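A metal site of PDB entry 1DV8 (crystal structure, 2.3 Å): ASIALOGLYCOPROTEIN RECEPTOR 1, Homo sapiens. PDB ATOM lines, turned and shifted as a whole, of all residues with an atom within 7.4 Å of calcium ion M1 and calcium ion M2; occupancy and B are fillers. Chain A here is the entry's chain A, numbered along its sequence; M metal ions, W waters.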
ATOM      1  N   HIS A  62      22.866  -9.713  22.238  1.00  0.00           N
ATOM      2  CA  HIS A  62      22.422 -10.507  23.377  1.00  0.00           C
ATOM      3  C   HIS A  62      20.979 -10.202  23.708  1.00  0.00           C
ATOM      4  O   HIS A  62      20.443  -9.162  23.278  1.00  0.00           O
ATOM      5  CB  HIS A  62      23.294 -10.199  24.609  1.00  0.00           C
ATOM      6  CG  HIS A  62      23.062  -8.823  25.163  1.00  0.00           C
ATOM      7  ND1 HIS A  62      22.100  -8.556  26.118  1.00  0.00           N
ATOM      8  CD2 HIS A  62      23.608  -7.630  24.842  1.00  0.00           C
ATOM      9  CE1 HIS A  62      22.052  -7.259  26.345  1.00  0.00           C
ATOM     10  NE2 HIS A  62      22.960  -6.667  25.578  1.00  0.00           N
ATOM     11  N   ASP A  63      20.344 -11.091  24.463  1.00  0.00           N
ATOM     12  CA  ASP A  63      18.972 -10.893  24.884  1.00  0.00           C
ATOM     13  C   ASP A  63      18.900 -11.063  26.401  1.00  0.00           C
ATOM     14  O   ASP A  63      17.901 -11.507  26.947  1.00  0.00           O
ATOM     15  CB  ASP A  63      18.028 -11.872  24.157  1.00  0.00           C
ATOM     16  CG  ASP A  63      18.126 -13.300  24.669  1.00  0.00           C
ATOM     17  OD1 ASP A  63      19.159 -13.646  25.282  1.00  0.00           O
ATOM     18  OD2 ASP A  63      17.159 -14.059  24.426  1.00  0.00           O
ATOM     19  N   GLN A  64      19.992 -10.685  27.057  1.00  0.00           N
ATOM     20  CA  GLN A  64      20.118 -10.775  28.506  1.00  0.00           C
ATOM     21  C   GLN A  64      19.119  -9.918  29.265  1.00  0.00           C
ATOM     22  O   GLN A  64      18.779 -10.235  30.411  1.00  0.00           O
ATOM     23  CB  GLN A  64      21.527 -10.356  28.932  1.00  0.00           C
ATOM     24  CG  GLN A  64      22.616 -11.391  28.701  1.00  0.00           C
ATOM     25  CD  GLN A  64      23.997 -10.756  28.635  1.00  0.00           C
ATOM     26  OE1 GLN A  64      24.395 -10.151  27.625  1.00  0.00           O
ATOM     27  NE2 GLN A  64      24.727 -10.877  29.724  1.00  0.00           N
ATOM     28  N   GLY A  66      16.147  -9.073  27.854  1.00  0.00           N
ATOM     29  CA  GLY A  66      14.850  -9.248  27.240  1.00  0.00           C
ATOM     30  C   GLY A  66      14.958  -9.350  25.732  1.00  0.00           C
ATOM     31  O   GLY A  66      15.284 -10.405  25.209  1.00  0.00           O
ATOM     32  N   TRP A  68      16.347  -8.771  21.771  1.00  0.00           N
ATOM     33  CA  TRP A  68      17.648  -8.730  21.144  1.00  0.00           C
ATOM     34  C   TRP A  68      18.071  -7.284  20.974  1.00  0.00           C
ATOM     35  O   TRP A  68      17.289  -6.445  20.516  1.00  0.00           O
ATOM     36  CB  TRP A  68      17.615  -9.453  19.797  1.00  0.00           C
ATOM     37  CG  TRP A  68      17.616 -10.944  19.946  1.00  0.00           C
ATOM     38  CD1 TRP A  68      16.565 -11.789  19.740  1.00  0.00           C
ATOM     39  CD2 TRP A  68      18.700 -11.756  20.418  1.00  0.00           C
ATOM     40  NE1 TRP A  68      16.930 -13.087  20.054  1.00  0.00           N
ATOM     41  CE2 TRP A  68      18.235 -13.091  20.474  1.00  0.00           C
ATOM     42  CE3 TRP A  68      20.019 -11.478  20.808  1.00  0.00           C
ATOM     43  CZ2 TRP A  68      19.037 -14.152  20.903  1.00  0.00           C
ATOM     44  CZ3 TRP A  68      20.825 -12.533  21.230  1.00  0.00           C
ATOM     45  CH2 TRP A  68      20.332 -13.858  21.279  1.00  0.00           C
ATOM     46  N   TRP A  83      21.091 -15.641  11.197  1.00  0.00           N
ATOM     47  CA  TRP A  83      20.985 -16.774  12.102  1.00  0.00           C
ATOM     48  C   TRP A  83      21.098 -18.118  11.401  1.00  0.00           C
ATOM     49  O   TRP A  83      20.755 -18.287  10.240  1.00  0.00           O
ATOM     50  CB  TRP A  83      19.653 -16.765  12.906  1.00  0.00           C
ATOM     51  CG  TRP A  83      19.461 -15.616  13.825  1.00  0.00           C
ATOM     52  CD1 TRP A  83      18.714 -14.499  13.594  1.00  0.00           C
ATOM     53  CD2 TRP A  83      20.034 -15.446  15.135  1.00  0.00           C
ATOM     54  NE1 TRP A  83      18.777 -13.655  14.665  1.00  0.00           N
ATOM     55  CE2 TRP A  83      19.577 -14.213  15.622  1.00  0.00           C
ATOM     56  CE3 TRP A  83      20.881 -16.234  15.932  1.00  0.00           C
ATOM     57  CZ2 TRP A  83      19.944 -13.730  16.868  1.00  0.00           C
ATOM     58  CZ3 TRP A  83      21.239 -15.748  17.175  1.00  0.00           C
ATOM     59  CH2 TRP A  83      20.768 -14.511  17.630  1.00  0.00           C
ATOM     60  N   GLU A  86      17.091 -22.756  12.709  1.00  0.00           N
ATOM     61  CA  GLU A  86      16.621 -23.205  14.014  1.00  0.00           C
ATOM     62  C   GLU A  86      17.243 -22.438  15.193  1.00  0.00           C
ATOM     63  O   GLU A  86      17.218 -22.909  16.326  1.00  0.00           O
ATOM     64  CB  GLU A  86      16.893 -24.694  14.181  1.00  0.00           C
ATOM     65  CG  GLU A  86      16.408 -25.530  13.006  1.00  0.00           C
ATOM     66  CD  GLU A  86      16.810 -26.988  13.128  1.00  0.00           C
ATOM     67  OE1 GLU A  86      16.172 -27.713  13.928  1.00  0.00           O
ATOM     68  OE2 GLU A  86      17.758 -27.405  12.418  1.00  0.00           O
ATOM     69  N   GLN A  87      17.814 -21.267  14.922  1.00  0.00           N
ATOM     70  CA  GLN A  87      18.389 -20.434  15.977  1.00  0.00           C
ATOM     71  C   GLN A  87      17.843 -19.013  15.804  1.00  0.00           C
ATOM     72  O   GLN A  87      17.492 -18.622  14.700  1.00  0.00           O
ATOM     73  CB  GLN A  87      19.918 -20.434  15.879  1.00  0.00           C
ATOM     74  CG  GLN A  87      20.567 -21.800  15.983  1.00  0.00           C
ATOM     75  CD  GLN A  87      20.333 -22.499  17.323  1.00  0.00           C
ATOM     76  OE1 GLN A  87      19.972 -21.887  18.331  1.00  0.00           O
ATOM     77  NE2 GLN A  87      20.560 -23.795  17.330  1.00  0.00           N
ATOM     78  N   PRO A  88      17.755 -18.238  16.893  1.00  0.00           N
ATOM     79  CA  PRO A  88      18.122 -18.570  18.275  1.00  0.00           C
ATOM     80  C   PRO A  88      17.132 -19.579  18.843  1.00  0.00           C
ATOM     81  O   PRO A  88      15.943 -19.549  18.492  1.00  0.00           O
ATOM     82  CB  PRO A  88      18.004 -17.222  19.003  1.00  0.00           C
ATOM     83  CG  PRO A  88      17.929 -16.186  17.911  1.00  0.00           C
ATOM     84  CD  PRO A  88      17.202 -16.880  16.792  1.00  0.00           C
ATOM     85  N   ASP A  89      17.598 -20.441  19.754  1.00  0.00           N
ATOM     86  CA  ASP A  89      16.711 -21.429  20.338  1.00  0.00           C
ATOM     87  C   ASP A  89      16.688 -21.427  21.880  1.00  0.00           C
ATOM     88  O   ASP A  89      16.021 -22.256  22.486  1.00  0.00           O
ATOM     89  CB  ASP A  89      17.080 -22.819  19.832  1.00  0.00           C
ATOM     90  CG  ASP A  89      18.375 -23.320  20.430  1.00  0.00           C
ATOM     91  OD1 ASP A  89      19.044 -22.495  21.097  1.00  0.00           O
ATOM     92  OD2 ASP A  89      18.731 -24.508  20.231  1.00  0.00           O
ATOM     93  N   ASP A  90      17.417 -20.506  22.490  1.00  0.00           N
ATOM     94  CA  ASP A  90      17.449 -20.377  23.955  1.00  0.00           C
ATOM     95  C   ASP A  90      17.488 -21.702  24.713  1.00  0.00           C
ATOM     96  O   ASP A  90      16.797 -21.873  25.723  1.00  0.00           O
ATOM     97  CB  ASP A  90      16.252 -19.538  24.442  1.00  0.00           C
ATOM     98  CG  ASP A  90      16.476 -18.895  25.825  1.00  0.00           C
ATOM     99  OD1 ASP A  90      17.514 -18.249  26.043  1.00  0.00           O
ATOM    100  OD2 ASP A  90      15.600 -19.023  26.703  1.00  0.00           O
ATOM    101  N   TRP A  91      18.319 -22.618  24.220  1.00  0.00           N
ATOM    102  CA  TRP A  91      18.491 -23.951  24.807  1.00  0.00           C
ATOM    103  C   TRP A  91      18.907 -23.978  26.293  1.00  0.00           C
ATOM    104  O   TRP A  91      19.734 -23.201  26.756  1.00  0.00           O
ATOM    105  CB  TRP A  91      19.534 -24.720  24.003  1.00  0.00           C
ATOM    106  CG  TRP A  91      19.606 -26.169  24.347  1.00  0.00           C
ATOM    107  CD1 TRP A  91      18.559 -27.030  24.491  1.00  0.00           C
ATOM    108  CD2 TRP A  91      20.806 -26.957  24.484  1.00  0.00           C
ATOM    109  NE1 TRP A  91      19.022 -28.311  24.691  1.00  0.00           N
ATOM    110  CE2 TRP A  91      20.394 -28.292  24.693  1.00  0.00           C
ATOM    111  CE3 TRP A  91      22.172 -26.664  24.439  1.00  0.00           C
ATOM    112  CZ2 TRP A  91      21.322 -29.345  24.862  1.00  0.00           C
ATOM    113  CZ3 TRP A  91      23.100 -27.718  24.608  1.00  0.00           C
ATOM    114  CH2 TRP A  91      22.661 -29.041  24.811  1.00  0.00           C
ATOM    115  N   TYR A  92      18.303 -24.909  27.030  1.00  0.00           N
ATOM    116  CA  TYR A  92      18.582 -25.106  28.446  1.00  0.00           C
ATOM    117  C   TYR A  92      19.275 -26.461  28.665  1.00  0.00           C
ATOM    118  O   TYR A  92      19.907 -26.668  29.704  1.00  0.00           O
ATOM    119  CB  TYR A  92      17.272 -25.090  29.267  1.00  0.00           C
ATOM    120  CG  TYR A  92      16.751 -23.715  29.639  1.00  0.00           C
ATOM    121  CD1 TYR A  92      16.260 -22.838  28.672  1.00  0.00           C
ATOM    122  CD2 TYR A  92      16.789 -23.275  30.969  1.00  0.00           C
ATOM    123  CE1 TYR A  92      15.798 -21.556  29.014  1.00  0.00           C
ATOM    124  CE2 TYR A  92      16.334 -21.995  31.327  1.00  0.00           C
ATOM    125  CZ  TYR A  92      15.848 -21.144  30.342  1.00  0.00           C
ATOM    126  OH  TYR A  92      15.394 -19.901  30.727  1.00  0.00           O
ATOM    127  N   GLY A  99      19.071 -20.245  29.958  1.00  0.00           N
ATOM    128  CA  GLY A  99      18.919 -20.569  28.551  1.00  0.00           C
ATOM    129  C   GLY A  99      20.203 -20.190  27.839  1.00  0.00           C
ATOM    130  O   GLY A  99      21.254 -20.627  28.263  1.00  0.00           O
ATOM    131  N   GLU A 100      20.102 -19.378  26.775  1.00  0.00           N
ATOM    132  CA  GLU A 100      21.255 -18.898  25.992  1.00  0.00           C
ATOM    133  C   GLU A 100      20.960 -17.442  25.579  1.00  0.00           C
ATOM    134  O   GLU A 100      20.019 -17.170  24.817  1.00  0.00           O
ATOM    135  CB  GLU A 100      21.450 -19.790  24.756  1.00  0.00           C
ATOM    136  CG  GLU A 100      21.934 -21.202  25.082  1.00  0.00           C
ATOM    137  CD  GLU A 100      21.959 -22.125  23.869  1.00  0.00           C
ATOM    138  OE1 GLU A 100      22.763 -23.078  23.831  1.00  0.00           O
ATOM    139  OE2 GLU A 100      21.163 -21.917  22.938  1.00  0.00           O
ATOM    140  N   ASP A 101      21.757 -16.514  26.091  1.00  0.00           N
ATOM    141  CA  ASP A 101      21.539 -15.103  25.848  1.00  0.00           C
ATOM    142  C   ASP A 101      22.601 -14.345  25.061  1.00  0.00           C
ATOM    143  O   ASP A 101      22.492 -13.147  24.898  1.00  0.00           O
ATOM    144  CB  ASP A 101      21.329 -14.392  27.182  1.00  0.00           C
ATOM    145  CG  ASP A 101      20.264 -15.048  28.008  1.00  0.00           C
ATOM    146  OD1 ASP A 101      19.402 -15.697  27.380  1.00  0.00           O
ATOM    147  OD2 ASP A 101      20.284 -14.901  29.259  1.00  0.00           O
ATOM    148  N   CYS A 102      23.634 -15.027  24.599  1.00  0.00           N
ATOM    149  CA  CYS A 102      24.662 -14.299  23.867  1.00  0.00           C
ATOM    150  C   CYS A 102      24.839 -14.893  22.485  1.00  0.00           C
ATOM    151  O   CYS A 102      24.878 -16.124  22.321  1.00  0.00           O
ATOM    152  CB  CYS A 102      25.962 -14.322  24.671  1.00  0.00           C
ATOM    153  SG  CYS A 102      25.876 -13.220  26.120  1.00  0.00           S
ATOM    154  N   HIS A 104      26.854 -15.611  18.949  1.00  0.00           N
ATOM    155  CA  HIS A 104      28.203 -15.817  18.467  1.00  0.00           C
ATOM    156  C   HIS A 104      28.165 -16.412  17.069  1.00  0.00           C
ATOM    157  O   HIS A 104      27.227 -17.119  16.687  1.00  0.00           O
ATOM    158  CB  HIS A 104      28.960 -16.753  19.416  1.00  0.00           C
ATOM    159  CG  HIS A 104      28.580 -18.198  19.290  1.00  0.00           C
ATOM    160  ND1 HIS A 104      29.210 -19.061  18.416  1.00  0.00           N
ATOM    161  CD2 HIS A 104      27.659 -18.941  19.956  1.00  0.00           C
ATOM    162  CE1 HIS A 104      28.704 -20.278  18.559  1.00  0.00           C
ATOM    163  NE2 HIS A 104      27.754 -20.230  19.484  1.00  0.00           N
ATOM    164  N   TRP A 111      25.004 -17.243  12.882  1.00  0.00           N
ATOM    165  CA  TRP A 111      24.881 -17.025  14.310  1.00  0.00           C
ATOM    166  C   TRP A 111      24.138 -18.089  15.101  1.00  0.00           C
ATOM    167  O   TRP A 111      23.305 -18.806  14.573  1.00  0.00           O
ATOM    168  CB  TRP A 111      24.233 -15.659  14.552  1.00  0.00           C
ATOM    169  CG  TRP A 111      24.709 -14.556  13.651  1.00  0.00           C
ATOM    170  CD1 TRP A 111      25.863 -14.514  12.947  1.00  0.00           C
ATOM    171  CD2 TRP A 111      24.060 -13.279  13.448  1.00  0.00           C
ATOM    172  NE1 TRP A 111      25.985 -13.299  12.310  1.00  0.00           N
ATOM    173  CE2 TRP A 111      24.892 -12.525  12.606  1.00  0.00           C
ATOM    174  CE3 TRP A 111      22.864 -12.716  13.894  1.00  0.00           C
ATOM    175  CZ2 TRP A 111      24.569 -11.224  12.205  1.00  0.00           C
ATOM    176  CZ3 TRP A 111      22.537 -11.421  13.501  1.00  0.00           C
ATOM    177  CH2 TRP A 111      23.387 -10.704  12.666  1.00  0.00           C
ATOM    178  N   ASN A 112      24.458 -18.172  16.382  1.00  0.00           N
ATOM    179  CA  ASN A 112      23.804 -19.098  17.304  1.00  0.00           C
ATOM    180  C   ASN A 112      23.821 -18.427  18.683  1.00  0.00           C
ATOM    181  O   ASN A 112      24.752 -17.690  19.002  1.00  0.00           O
ATOM    182  CB  ASN A 112      24.559 -20.430  17.380  1.00  0.00           C
ATOM    183  CG  ASN A 112      24.049 -21.320  18.504  1.00  0.00           C
ATOM    184  OD1 ASN A 112      22.845 -21.464  18.712  1.00  0.00           O
ATOM    185  ND2 ASN A 112      24.972 -21.921  19.227  1.00  0.00           N
ATOM    186  N   ASP A 113      22.784 -18.648  19.485  1.00  0.00           N
ATOM    187  CA  ASP A 113      22.763 -18.070  20.825  1.00  0.00           C
ATOM    188  C   ASP A 113      23.286 -19.191  21.724  1.00  0.00           C
ATOM    189  O   ASP A 113      22.934 -20.347  21.526  1.00  0.00           O
ATOM    190  CB  ASP A 113      21.344 -17.644  21.211  1.00  0.00           C
ATOM    191  CG  ASP A 113      20.350 -18.798  21.203  1.00  0.00           C
ATOM    192  OD1 ASP A 113      20.636 -19.828  20.555  1.00  0.00           O
ATOM    193  OD2 ASP A 113      19.257 -18.641  21.822  1.00  0.00           O
ATOM    194  N   ASP A 114      24.136 -18.834  22.694  1.00  0.00           N
ATOM    195  CA  ASP A 114      24.747 -19.814  23.586  1.00  0.00           C
ATOM    196  C   ASP A 114      24.927 -19.213  24.995  1.00  0.00           C
ATOM    197  O   ASP A 114      24.703 -18.015  25.201  1.00  0.00           O
ATOM    198  CB  ASP A 114      26.117 -20.223  23.008  1.00  0.00           C
ATOM    199  CG  ASP A 114      26.568 -21.586  23.468  1.00  0.00           C
ATOM    200  OD1 ASP A 114      27.413 -22.205  22.777  1.00  0.00           O
ATOM    201  OD2 ASP A 114      26.080 -22.054  24.526  1.00  0.00           O
ATOM    202  N   VAL A 115      25.353 -20.044  25.938  1.00  0.00           N
ATOM    203  CA  VAL A 115      25.560 -19.667  27.334  1.00  0.00           C
ATOM    204  C   VAL A 115      26.615 -18.584  27.440  1.00  0.00           C
ATOM    205  O   VAL A 115      27.788 -18.819  27.162  1.00  0.00           O
ATOM    206  CB  VAL A 115      25.981 -20.895  28.163  1.00  0.00           C
ATOM    207  CG1 VAL A 115      26.288 -20.495  29.588  1.00  0.00           C
ATOM    208  CG2 VAL A 115      24.871 -21.937  28.128  1.00  0.00           C
HETATM  209 CA    CA M   1      17.903 -16.020  25.598  1.00  0.00          CA
HETATM  210 CA    CA M   2      21.405 -21.980  20.589  1.00  0.00          CA
HETATM  211  O   HOH W   1      16.554 -15.448  27.302  1.00  0.00           O
HETATM  212  O   HOH W   2      21.320 -24.750  20.262  1.00  0.00           O
HETATM  213  O   HOH W   3      23.344 -24.136  21.403  1.00  0.00           O
HETATM  214  O   HOH W   4      17.820 -16.830  23.435  1.00  0.00           O
HETATM  215  O   HOH W   5      15.770 -16.236  24.941  1.00  0.00           O
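Calcium ion M2 is bound by OD1 of Asp 113 (2.3 Å), OE2 of Glu 100 (2.4 Å), OD1 of Asn 112 (2.4 Å), O of Asp 113 (2.4 Å), OD1 of Asp 89 (2.5 Å), OE1 of Gln 87 (2.7 Å) and water W2 (2.8 Å). Slightly farther from calcium ion M2 lies water W3 (3.0 Å).
Water W2 bridges the side-chain carboxylate (OD2) of Asp 89 and the side-chain amide nitrogen (NE2) of Gln 87.
OD2 of Asp 113 lies within hydrogen-bond range of N of Asp 90 (2.7 Å). The backbone carbonyl oxygen of Asp 114 is in hydrogen-bond range of the backbone NH of Asp 101, at 3.4 Å. The backbone NH (N) of Trp 91 lies close to the side-chain carboxylate (OE2) of Glu 100 (3.2 Å). O of Asn 112 sits at hydrogen-bond distance from N of His 104 (3.0 Å). The side-chain carboxylate of Asp 89 sits close to the backbone NH of Trp 91 (3.2 Å).
Four residues have an atom within 4 Å of calcium ion M1: Asp 63, Asp 90, Glu 100 and Asp 101. The nearest printed residue that does not touch calcium ion M1 is Asp 113 (4.8 Å).
Calcium ion M1 is bound by water W5, at 2.2 Å. Water W1 is bound to calcium ion M1 (2.2 Å). OD1 of Asp 90 binds calcium ion M1, at 2.3 Å. Water W4 is bound to calcium ion M1, 2.3 Å away. Calcium ion M1 is bound by OD1 of Asp 101 (2.4 Å). OD2 of Asp 63 is bound to calcium ion M1 (2.4 Å). The backbone carbonyl oxygen (O) of Glu 100 binds calcium ion M1 (2.5 Å). Calcium ion M1 is bound by OD1 of Asp 63 (2.7 Å).
Of the 23 residues printed, 5 come within 4 Å of calcium ion M2.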
